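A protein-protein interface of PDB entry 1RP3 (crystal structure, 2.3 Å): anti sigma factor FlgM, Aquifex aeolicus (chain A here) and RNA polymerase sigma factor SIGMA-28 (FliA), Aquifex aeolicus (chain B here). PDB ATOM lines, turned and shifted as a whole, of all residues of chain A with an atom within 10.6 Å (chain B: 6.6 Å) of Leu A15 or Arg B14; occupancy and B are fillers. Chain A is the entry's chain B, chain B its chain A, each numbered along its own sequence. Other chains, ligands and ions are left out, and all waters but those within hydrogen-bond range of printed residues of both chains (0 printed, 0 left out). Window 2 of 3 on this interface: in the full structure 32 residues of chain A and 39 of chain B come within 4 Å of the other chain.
The backbone carbonyl oxygen (O) of Leu A14 sits at hydrogen-bond distance from the side-chain hydroxyl (OG1) of Thr A17 (2.9 Å).
NE of Arg B14 lies within salt-bridge range of OD1 of Asp B58, at 2.7 Å.
Among the printed residues, pairs that only touch across the chains: Ile A11 with Leu B19, Ile A11 with Ile B18, Leu A7 with Leu B19, Leu A15 with Glu B15, Ile A11 with Glu B15, Leu A15 with Ile B18, Leu A14 with Ile B54, Leu A15 with Arg B14, Ser A8 with Leu B19 and Leu A15 with Ile B54.
Arg B14 touches just one residue of chain A: Leu A15.
Of chain A, only Ile A11 and Leu A15 come within 4 Å of Ile B18.
Of the printed residues of chain B, Leu A14 touches Ile B54 (3.9 Å).
Of the printed residues of chain A, Ile B54 touches Leu A14 and Leu A15.
The nearest residue of chain A that does not touch Arg B14 is Ile A11 (6.4 Å).
Hydrophobic or aromatic side chains of chain A that line the printed part of chain B: Leu A7, Ile A11, Leu A14 and Leu A15.
Of the 15 printed residues of chain B, 5 touch a printed residue of chain A.
Among the printed residues, 10 pairs touch across the chains.
Among the printed residues, no Asp or Glu carboxylate lies within 4 Å of a Lys or Arg side-chain nitrogen of the other chain.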
ATOM      1  N   LEU A   7     -23.496   0.852  26.314  1.00  0.00           N
ATOM      2  CA  LEU A   7     -22.526   0.878  25.223  1.00  0.00           C
ATOM      3  C   LEU A   7     -21.649  -0.367  25.254  1.00  0.00           C
ATOM      4  O   LEU A   7     -21.455  -1.019  24.226  1.00  0.00           O
ATOM      5  CB  LEU A   7     -21.660   2.142  25.286  1.00  0.00           C
ATOM      6  CG  LEU A   7     -22.357   3.455  24.913  1.00  0.00           C
ATOM      7  CD1 LEU A   7     -21.412   4.639  25.045  1.00  0.00           C
ATOM      8  CD2 LEU A   7     -22.880   3.345  23.497  1.00  0.00           C
ATOM      9  N   SER A   8     -21.162  -0.715  26.445  1.00  0.00           N
ATOM     10  CA  SER A   8     -20.309  -1.888  26.633  1.00  0.00           C
ATOM     11  C   SER A   8     -21.041  -3.158  26.232  1.00  0.00           C
ATOM     12  O   SER A   8     -20.455  -4.076  25.676  1.00  0.00           O
ATOM     13  CB  SER A   8     -19.858  -1.981  28.095  1.00  0.00           C
ATOM     14  OG  SER A   8     -19.062  -3.132  28.311  1.00  0.00           O
ATOM     15  N   ARG A   9     -22.341  -3.188  26.490  1.00  0.00           N
ATOM     16  CA  ARG A   9     -23.147  -4.350  26.159  1.00  0.00           C
ATOM     17  C   ARG A   9     -23.336  -4.430  24.655  1.00  0.00           C
ATOM     18  O   ARG A   9     -23.203  -5.501  24.060  1.00  0.00           O
ATOM     19  CB  ARG A   9     -24.510  -4.279  26.861  1.00  0.00           C
ATOM     20  CG  ARG A   9     -25.284  -5.601  26.839  1.00  0.00           C
ATOM     21  CD  ARG A   9     -26.797  -5.390  26.946  1.00  0.00           C
ATOM     22  NE  ARG A   9     -27.480  -5.716  25.691  1.00  0.00           N
ATOM     23  CZ  ARG A   9     -28.298  -4.892  25.042  1.00  0.00           C
ATOM     24  NH1 ARG A   9     -28.545  -3.680  25.525  1.00  0.00           N
ATOM     25  NH2 ARG A   9     -28.859  -5.276  23.899  1.00  0.00           N
ATOM     26  N   LEU A  10     -23.610  -3.282  24.041  1.00  0.00           N
ATOM     27  CA  LEU A  10     -23.820  -3.201  22.602  1.00  0.00           C
ATOM     28  C   LEU A  10     -22.564  -3.581  21.836  1.00  0.00           C
ATOM     29  O   LEU A  10     -22.637  -4.326  20.863  1.00  0.00           O
ATOM     30  CB  LEU A  10     -24.324  -1.808  22.207  1.00  0.00           C
ATOM     31  CG  LEU A  10     -25.791  -1.563  22.585  1.00  0.00           C
ATOM     32  CD1 LEU A  10     -26.152  -0.107  22.423  1.00  0.00           C
ATOM     33  CD2 LEU A  10     -26.692  -2.450  21.747  1.00  0.00           C
ATOM     34  N   ILE A  11     -21.410  -3.107  22.304  1.00  0.00           N
ATOM     35  CA  ILE A  11     -20.125  -3.431  21.685  1.00  0.00           C
ATOM     36  C   ILE A  11     -19.904  -4.943  21.753  1.00  0.00           C
ATOM     37  O   ILE A  11     -19.418  -5.561  20.797  1.00  0.00           O
ATOM     38  CB  ILE A  11     -18.959  -2.685  22.377  1.00  0.00           C
ATOM     39  CG1 ILE A  11     -18.975  -1.210  21.973  1.00  0.00           C
ATOM     40  CG2 ILE A  11     -17.621  -3.285  21.978  1.00  0.00           C
ATOM     41  CD1 ILE A  11     -17.906  -0.400  22.626  1.00  0.00           C
ATOM     42  N   GLY A  12     -20.323  -5.534  22.874  1.00  0.00           N
ATOM     43  CA  GLY A  12     -20.213  -6.970  23.070  1.00  0.00           C
ATOM     44  C   GLY A  12     -20.970  -7.766  22.020  1.00  0.00           C
ATOM     45  O   GLY A  12     -20.473  -8.789  21.545  1.00  0.00           O
ATOM     46  N   LEU A  13     -22.161  -7.289  21.640  1.00  0.00           N
ATOM     47  CA  LEU A  13     -22.983  -7.965  20.623  1.00  0.00           C
ATOM     48  C   LEU A  13     -22.315  -7.848  19.265  1.00  0.00           C
ATOM     49  O   LEU A  13     -22.304  -8.792  18.477  1.00  0.00           O
ATOM     50  CB  LEU A  13     -24.389  -7.350  20.538  1.00  0.00           C
ATOM     51  CG  LEU A  13     -25.279  -7.425  21.775  1.00  0.00           C
ATOM     52  CD1 LEU A  13     -26.683  -6.998  21.388  1.00  0.00           C
ATOM     53  CD2 LEU A  13     -25.300  -8.846  22.321  1.00  0.00           C
ATOM     54  N   LEU A  14     -21.736  -6.680  19.023  1.00  0.00           N
ATOM     55  CA  LEU A  14     -21.057  -6.372  17.778  1.00  0.00           C
ATOM     56  C   LEU A  14     -19.827  -7.251  17.579  1.00  0.00           C
ATOM     57  O   LEU A  14     -19.675  -7.882  16.528  1.00  0.00           O
ATOM     58  CB  LEU A  14     -20.639  -4.905  17.800  1.00  0.00           C
ATOM     59  CG  LEU A  14     -20.717  -4.095  16.520  1.00  0.00           C
ATOM     60  CD1 LEU A  14     -22.077  -4.264  15.870  1.00  0.00           C
ATOM     61  CD2 LEU A  14     -20.442  -2.644  16.865  1.00  0.00           C
ATOM     62  N   LEU A  15     -18.961  -7.289  18.593  1.00  0.00           N
ATOM     63  CA  LEU A  15     -17.725  -8.068  18.557  1.00  0.00           C
ATOM     64  C   LEU A  15     -17.914  -9.577  18.680  1.00  0.00           C
ATOM     65  O   LEU A  15     -16.937 -10.329  18.594  1.00  0.00           O
ATOM     66  CB  LEU A  15     -16.739  -7.571  19.622  1.00  0.00           C
ATOM     67  CG  LEU A  15     -15.883  -6.344  19.274  1.00  0.00           C
ATOM     68  CD1 LEU A  15     -16.747  -5.183  18.830  1.00  0.00           C
ATOM     69  CD2 LEU A  15     -15.037  -5.950  20.466  1.00  0.00           C
ATOM     70  N   GLU A  16     -19.147 -10.018  18.926  1.00  0.00           N
ATOM     71  CA  GLU A  16     -19.438 -11.449  19.012  1.00  0.00           C
ATOM     72  C   GLU A  16     -19.771 -12.047  17.632  1.00  0.00           C
ATOM     73  O   GLU A  16     -19.833 -13.268  17.484  1.00  0.00           O
ATOM     74  CB  GLU A  16     -20.578 -11.685  19.966  1.00  0.00           C
ATOM     75  N   THR A  17     -20.004 -11.182  16.641  1.00  0.00           N
ATOM     76  CA  THR A  17     -20.311 -11.609  15.271  1.00  0.00           C
ATOM     77  C   THR A  17     -19.087 -11.353  14.391  1.00  0.00           C
ATOM     78  O   THR A  17     -19.073 -11.685  13.213  1.00  0.00           O
ATOM     79  CB  THR A  17     -21.521 -10.841  14.663  1.00  0.00           C
ATOM     80  OG1 THR A  17     -21.264  -9.433  14.687  1.00  0.00           O
ATOM     81  CG2 THR A  17     -22.807 -11.132  15.435  1.00  0.00           C
ATOM     82  N   SER A  28     -24.018 -17.895  15.186  1.00  0.00           N
ATOM     83  CA  SER A  28     -23.851 -16.662  14.425  1.00  0.00           C
ATOM     84  C   SER A  28     -24.935 -15.629  14.775  1.00  0.00           C
ATOM     85  O   SER A  28     -24.913 -15.029  15.854  1.00  0.00           O
ATOM     86  CB  SER A  28     -23.855 -16.969  12.920  1.00  0.00           C
ATOM     87  OG  SER A  28     -25.067 -17.590  12.515  1.00  0.00           O
ATOM     88  N   ASN A  31     -24.679 -11.506  10.586  1.00  0.00           N
ATOM     89  CA  ASN A  31     -23.968 -10.235  10.761  1.00  0.00           C
ATOM     90  C   ASN A  31     -24.639  -8.947  10.274  1.00  0.00           C
ATOM     91  O   ASN A  31     -25.398  -8.330  11.022  1.00  0.00           O
ATOM     92  CB  ASN A  31     -22.550 -10.348  10.174  1.00  0.00           C
ATOM     93  N   GLU A  34     -28.115  -7.933  11.750  1.00  0.00           N
ATOM     94  CA  GLU A  34     -28.075  -7.696  13.186  1.00  0.00           C
ATOM     95  C   GLU A  34     -27.226  -6.483  13.548  1.00  0.00           C
ATOM     96  O   GLU A  34     -27.626  -5.654  14.365  1.00  0.00           O
ATOM     97  CB  GLU A  34     -27.510  -8.913  13.909  1.00  0.00           C
ATOM     98  CG  GLU A  34     -28.538  -9.923  14.370  1.00  0.00           C
ATOM     99  CD  GLU A  34     -27.960 -10.938  15.356  1.00  0.00           C
ATOM    100  OE1 GLU A  34     -26.818 -10.751  15.833  1.00  0.00           O
ATOM    101  OE2 GLU A  34     -28.659 -11.927  15.661  1.00  0.00           O
ATOM    102  N   ASP A  35     -26.054  -6.385  12.928  1.00  0.00           N
ATOM    103  CA  ASP A  35     -25.130  -5.295  13.194  1.00  0.00           C
ATOM    104  C   ASP A  35     -25.682  -3.924  12.836  1.00  0.00           C
ATOM    105  O   ASP A  35     -25.432  -2.950  13.550  1.00  0.00           O
ATOM    106  CB  ASP A  35     -23.788  -5.563  12.514  1.00  0.00           C
ATOM    107  CG  ASP A  35     -23.072  -6.778  13.091  1.00  0.00           C
ATOM    108  OD1 ASP A  35     -23.541  -7.329  14.114  1.00  0.00           O
ATOM    109  OD2 ASP A  35     -22.033  -7.183  12.522  1.00  0.00           O
ATOM    110  N   THR A  38     -27.646  -3.033  15.840  1.00  0.00           N
ATOM    111  CA  THR A  38     -26.765  -2.791  16.974  1.00  0.00           C
ATOM    112  C   THR A  38     -26.040  -1.452  16.794  1.00  0.00           C
ATOM    113  O   THR A  38     -25.972  -0.652  17.725  1.00  0.00           O
ATOM    114  CB  THR A  38     -25.753  -3.930  17.116  1.00  0.00           C
ATOM    115  OG1 THR A  38     -26.455  -5.168  17.237  1.00  0.00           O
ATOM    116  CG2 THR A  38     -24.887  -3.736  18.329  1.00  0.00           C
ATOM    117  N   LEU A  39     -25.531  -1.206  15.584  1.00  0.00           N
ATOM    118  CA  LEU A  39     -24.828   0.042  15.277  1.00  0.00           C
ATOM    119  C   LEU A  39     -25.755   1.232  15.471  1.00  0.00           C
ATOM    120  O   LEU A  39     -25.350   2.265  16.033  1.00  0.00           O
ATOM    121  CB  LEU A  39     -24.270   0.014  13.849  1.00  0.00           C
ATOM    122  CG  LEU A  39     -23.015  -0.861  13.698  1.00  0.00           C
ATOM    123  CD1 LEU A  39     -22.720  -1.186  12.228  1.00  0.00           C
ATOM    124  CD2 LEU A  39     -21.839  -0.171  14.351  1.00  0.00           C
ATOM    125  N   ILE A  42     -26.116   1.916  19.139  1.00  0.00           N
ATOM    126  CA  ILE A  42     -24.925   2.582  19.659  1.00  0.00           C
ATOM    127  C   ILE A  42     -25.015   4.077  19.316  1.00  0.00           C
ATOM    128  O   ILE A  42     -24.760   4.924  20.172  1.00  0.00           O
ATOM    129  CB  ILE A  42     -23.612   1.970  19.089  1.00  0.00           C
ATOM    130  CG1 ILE A  42     -23.439   0.539  19.598  1.00  0.00           C
ATOM    131  CG2 ILE A  42     -22.396   2.837  19.473  1.00  0.00           C
ATOM    132  CD1 ILE A  42     -22.205  -0.161  19.080  1.00  0.00           C
ATOM    133  N   SER B   9      -7.631 -10.553  28.473  1.00  0.00           N
ATOM    134  CA  SER B   9      -6.999  -9.251  28.503  1.00  0.00           C
ATOM    135  C   SER B   9      -7.081  -8.546  27.148  1.00  0.00           C
ATOM    136  O   SER B   9      -7.521  -7.403  27.075  1.00  0.00           O
ATOM    137  CB  SER B   9      -5.545  -9.392  28.961  1.00  0.00           C
ATOM    138  OG  SER B   9      -5.489  -9.896  30.289  1.00  0.00           O
ATOM    139  N   ASN B  10      -6.689  -9.238  26.079  1.00  0.00           N
ATOM    140  CA  ASN B  10      -6.738  -8.662  24.739  1.00  0.00           C
ATOM    141  C   ASN B  10      -8.149  -8.176  24.429  1.00  0.00           C
ATOM    142  O   ASN B  10      -8.333  -7.049  23.968  1.00  0.00           O
ATOM    143  CB  ASN B  10      -6.272  -9.668  23.673  1.00  0.00           C
ATOM    144  CG  ASN B  10      -4.746  -9.784  23.600  1.00  0.00           C
ATOM    145  OD1 ASN B  10      -4.041  -8.781  23.678  1.00  0.00           O
ATOM    146  ND2 ASN B  10      -4.235 -11.007  23.450  1.00  0.00           N
ATOM    147  N   GLN B  11      -9.134  -9.005  24.753  1.00  0.00           N
ATOM    148  CA  GLN B  11     -10.534  -8.696  24.519  1.00  0.00           C
ATOM    149  C   GLN B  11     -10.971  -7.413  25.225  1.00  0.00           C
ATOM    150  O   GLN B  11     -11.585  -6.531  24.608  1.00  0.00           O
ATOM    151  CB  GLN B  11     -11.394  -9.869  24.981  1.00  0.00           C
ATOM    152  CG  GLN B  11     -12.891  -9.628  24.961  1.00  0.00           C
ATOM    153  CD  GLN B  11     -13.679 -10.843  25.438  1.00  0.00           C
ATOM    154  OE1 GLN B  11     -13.427 -11.388  26.520  1.00  0.00           O
ATOM    155  NE2 GLN B  11     -14.641 -11.275  24.627  1.00  0.00           N
ATOM    156  N   ILE B  12     -10.637  -7.311  26.509  1.00  0.00           N
ATOM    157  CA  ILE B  12     -10.997  -6.155  27.316  1.00  0.00           C
ATOM    158  C   ILE B  12     -10.284  -4.887  26.868  1.00  0.00           C
ATOM    159  O   ILE B  12     -10.912  -3.833  26.756  1.00  0.00           O
ATOM    160  CB  ILE B  12     -10.728  -6.414  28.833  1.00  0.00           C
ATOM    161  CG1 ILE B  12     -11.642  -7.529  29.340  1.00  0.00           C
ATOM    162  CG2 ILE B  12     -10.949  -5.146  29.670  1.00  0.00           C
ATOM    163  CD1 ILE B  12     -13.119  -7.260  29.128  1.00  0.00           C
ATOM    164  N   GLU B  13      -8.978  -4.980  26.628  1.00  0.00           N
ATOM    165  CA  GLU B  13      -8.213  -3.809  26.198  1.00  0.00           C
ATOM    166  C   GLU B  13      -8.866  -3.225  24.947  1.00  0.00           C
ATOM    167  O   GLU B  13      -9.052  -2.014  24.842  1.00  0.00           O
ATOM    168  CB  GLU B  13      -6.748  -4.161  25.892  1.00  0.00           C
ATOM    169  CG  GLU B  13      -5.956  -4.860  27.014  1.00  0.00           C
ATOM    170  CD  GLU B  13      -5.848  -4.066  28.307  1.00  0.00           C
ATOM    171  OE1 GLU B  13      -6.114  -2.842  28.303  1.00  0.00           O
ATOM    172  OE2 GLU B  13      -5.480  -4.679  29.337  1.00  0.00           O
ATOM    173  N   ARG B  14      -9.252  -4.111  24.032  1.00  0.00           N
ATOM    174  CA  ARG B  14      -9.888  -3.745  22.782  1.00  0.00           C
ATOM    175  C   ARG B  14     -11.205  -2.990  23.035  1.00  0.00           C
ATOM    176  O   ARG B  14     -11.384  -1.864  22.548  1.00  0.00           O
ATOM    177  CB  ARG B  14     -10.132  -5.017  21.965  1.00  0.00           C
ATOM    178  CG  ARG B  14     -10.658  -4.805  20.555  1.00  0.00           C
ATOM    179  CD  ARG B  14     -10.937  -6.140  19.893  1.00  0.00           C
ATOM    180  NE  ARG B  14     -11.487  -5.994  18.549  1.00  0.00           N
ATOM    181  CZ  ARG B  14     -12.182  -6.932  17.916  1.00  0.00           C
ATOM    182  NH1 ARG B  14     -12.420  -8.099  18.504  1.00  0.00           N
ATOM    183  NH2 ARG B  14     -12.631  -6.709  16.687  1.00  0.00           N
ATOM    184  N   GLU B  15     -12.091  -3.575  23.843  1.00  0.00           N
ATOM    185  CA  GLU B  15     -13.376  -2.941  24.145  1.00  0.00           C
ATOM    186  C   GLU B  15     -13.238  -1.584  24.810  1.00  0.00           C
ATOM    187  O   GLU B  15     -13.935  -0.637  24.449  1.00  0.00           O
ATOM    188  CB  GLU B  15     -14.278  -3.864  24.960  1.00  0.00           C
ATOM    189  CG  GLU B  15     -14.865  -4.958  24.082  1.00  0.00           C
ATOM    190  CD  GLU B  15     -15.707  -5.991  24.822  1.00  0.00           C
ATOM    191  OE1 GLU B  15     -16.249  -5.676  25.914  1.00  0.00           O
ATOM    192  OE2 GLU B  15     -15.833  -7.119  24.281  1.00  0.00           O
ATOM    193  N   GLU B  16     -12.326  -1.486  25.763  1.00  0.00           N
ATOM    194  CA  GLU B  16     -12.093  -0.231  26.452  1.00  0.00           C
ATOM    195  C   GLU B  16     -11.621   0.815  25.454  1.00  0.00           C
ATOM    196  O   GLU B  16     -12.000   1.982  25.530  1.00  0.00           O
ATOM    197  CB  GLU B  16     -11.033  -0.403  27.545  1.00  0.00           C
ATOM    198  CG  GLU B  16     -11.479  -1.234  28.751  1.00  0.00           C
ATOM    199  CD  GLU B  16     -12.699  -0.663  29.456  1.00  0.00           C
ATOM    200  OE1 GLU B  16     -12.863   0.584  29.462  1.00  0.00           O
ATOM    201  OE2 GLU B  16     -13.489  -1.465  30.006  1.00  0.00           O
ATOM    202  N   LEU B  17     -10.790   0.378  24.510  1.00  0.00           N
ATOM    203  CA  LEU B  17     -10.244   1.268  23.489  1.00  0.00           C
ATOM    204  C   LEU B  17     -11.385   1.764  22.577  1.00  0.00           C
ATOM    205  O   LEU B  17     -11.495   2.958  22.316  1.00  0.00           O
ATOM    206  CB  LEU B  17      -9.137   0.542  22.713  1.00  0.00           C
ATOM    207  CG  LEU B  17      -7.900   1.306  22.210  1.00  0.00           C
ATOM    208  CD1 LEU B  17      -7.367   2.288  23.250  1.00  0.00           C
ATOM    209  CD2 LEU B  17      -6.814   0.296  21.845  1.00  0.00           C
ATOM    210  N   ILE B  18     -12.275   0.858  22.173  1.00  0.00           N
ATOM    211  CA  ILE B  18     -13.418   1.210  21.336  1.00  0.00           C
ATOM    212  C   ILE B  18     -14.290   2.201  22.090  1.00  0.00           C
ATOM    213  O   ILE B  18     -14.558   3.305  21.615  1.00  0.00           O
ATOM    214  CB  ILE B  18     -14.253  -0.043  20.954  1.00  0.00           C
ATOM    215  CG1 ILE B  18     -13.420  -0.971  20.069  1.00  0.00           C
ATOM    216  CG2 ILE B  18     -15.521   0.355  20.213  1.00  0.00           C
ATOM    217  CD1 ILE B  18     -14.111  -2.282  19.730  1.00  0.00           C
ATOM    218  N   LEU B  19     -14.682   1.807  23.296  1.00  0.00           N
ATOM    219  CA  LEU B  19     -15.507   2.621  24.180  1.00  0.00           C
ATOM    220  C   LEU B  19     -14.908   4.011  24.345  1.00  0.00           C
ATOM    221  O   LEU B  19     -15.608   5.008  24.223  1.00  0.00           O
ATOM    222  CB  LEU B  19     -15.581   1.943  25.548  1.00  0.00           C
ATOM    223  CG  LEU B  19     -16.876   1.835  26.347  1.00  0.00           C
ATOM    224  CD1 LEU B  19     -18.039   1.449  25.453  1.00  0.00           C
ATOM    225  CD2 LEU B  19     -16.671   0.771  27.438  1.00  0.00           C
ATOM    226  N   ILE B  54     -13.391   0.387  14.985  1.00  0.00           N
ATOM    227  CA  ILE B  54     -13.047  -0.970  15.387  1.00  0.00           C
ATOM    228  C   ILE B  54     -11.901  -1.519  14.541  1.00  0.00           C
ATOM    229  O   ILE B  54     -11.022  -2.200  15.052  1.00  0.00           O
ATOM    230  CB  ILE B  54     -14.268  -1.908  15.271  1.00  0.00           C
ATOM    231  CG1 ILE B  54     -15.356  -1.472  16.251  1.00  0.00           C
ATOM    232  CG2 ILE B  54     -13.859  -3.357  15.510  1.00  0.00           C
ATOM    233  CD1 ILE B  54     -16.671  -2.265  16.112  1.00  0.00           C
ATOM    234  N   LYS B  55     -11.940  -1.248  13.241  1.00  0.00           N
ATOM    235  CA  LYS B  55     -10.892  -1.703  12.338  1.00  0.00           C
ATOM    236  C   LYS B  55      -9.553  -1.047  12.649  1.00  0.00           C
ATOM    237  O   LYS B  55      -8.522  -1.718  12.624  1.00  0.00           O
ATOM    238  CB  LYS B  55     -11.282  -1.457  10.887  1.00  0.00           C
ATOM    239  CG  LYS B  55     -12.361  -2.406  10.397  1.00  0.00           C
ATOM    240  CD  LYS B  55     -12.733  -2.101   8.957  1.00  0.00           C
ATOM    241  CE  LYS B  55     -13.738  -3.104   8.413  1.00  0.00           C
ATOM    242  NZ  LYS B  55     -14.242  -2.673   7.062  1.00  0.00           N
ATOM    243  N   VAL B  57      -8.614   0.107  15.571  1.00  0.00           N
ATOM    244  CA  VAL B  57      -8.143  -0.424  16.847  1.00  0.00           C
ATOM    245  C   VAL B  57      -7.440  -1.770  16.664  1.00  0.00           C
ATOM    246  O   VAL B  57      -6.392  -2.014  17.255  1.00  0.00           O
ATOM    247  CB  VAL B  57      -9.308  -0.552  17.854  1.00  0.00           C
ATOM    248  CG1 VAL B  57      -8.922  -1.440  19.038  1.00  0.00           C
ATOM    249  CG2 VAL B  57      -9.696   0.819  18.342  1.00  0.00           C
ATOM    250  N   ASP B  58      -7.987  -2.604  15.790  1.00  0.00           N
ATOM    251  CA  ASP B  58      -7.424  -3.917  15.535  1.00  0.00           C
ATOM    252  C   ASP B  58      -6.088  -3.866  14.805  1.00  0.00           C
ATOM    253  O   ASP B  58      -5.187  -4.655  15.098  1.00  0.00           O
ATOM    254  CB  ASP B  58      -8.417  -4.783  14.745  1.00  0.00           C
ATOM    255  CG  ASP B  58      -9.663  -5.138  15.548  1.00  0.00           C
ATOM    256  OD1 ASP B  58      -9.682  -4.910  16.780  1.00  0.00           O
ATOM    257  OD2 ASP B  58     -10.628  -5.657  14.939  1.00  0.00           O
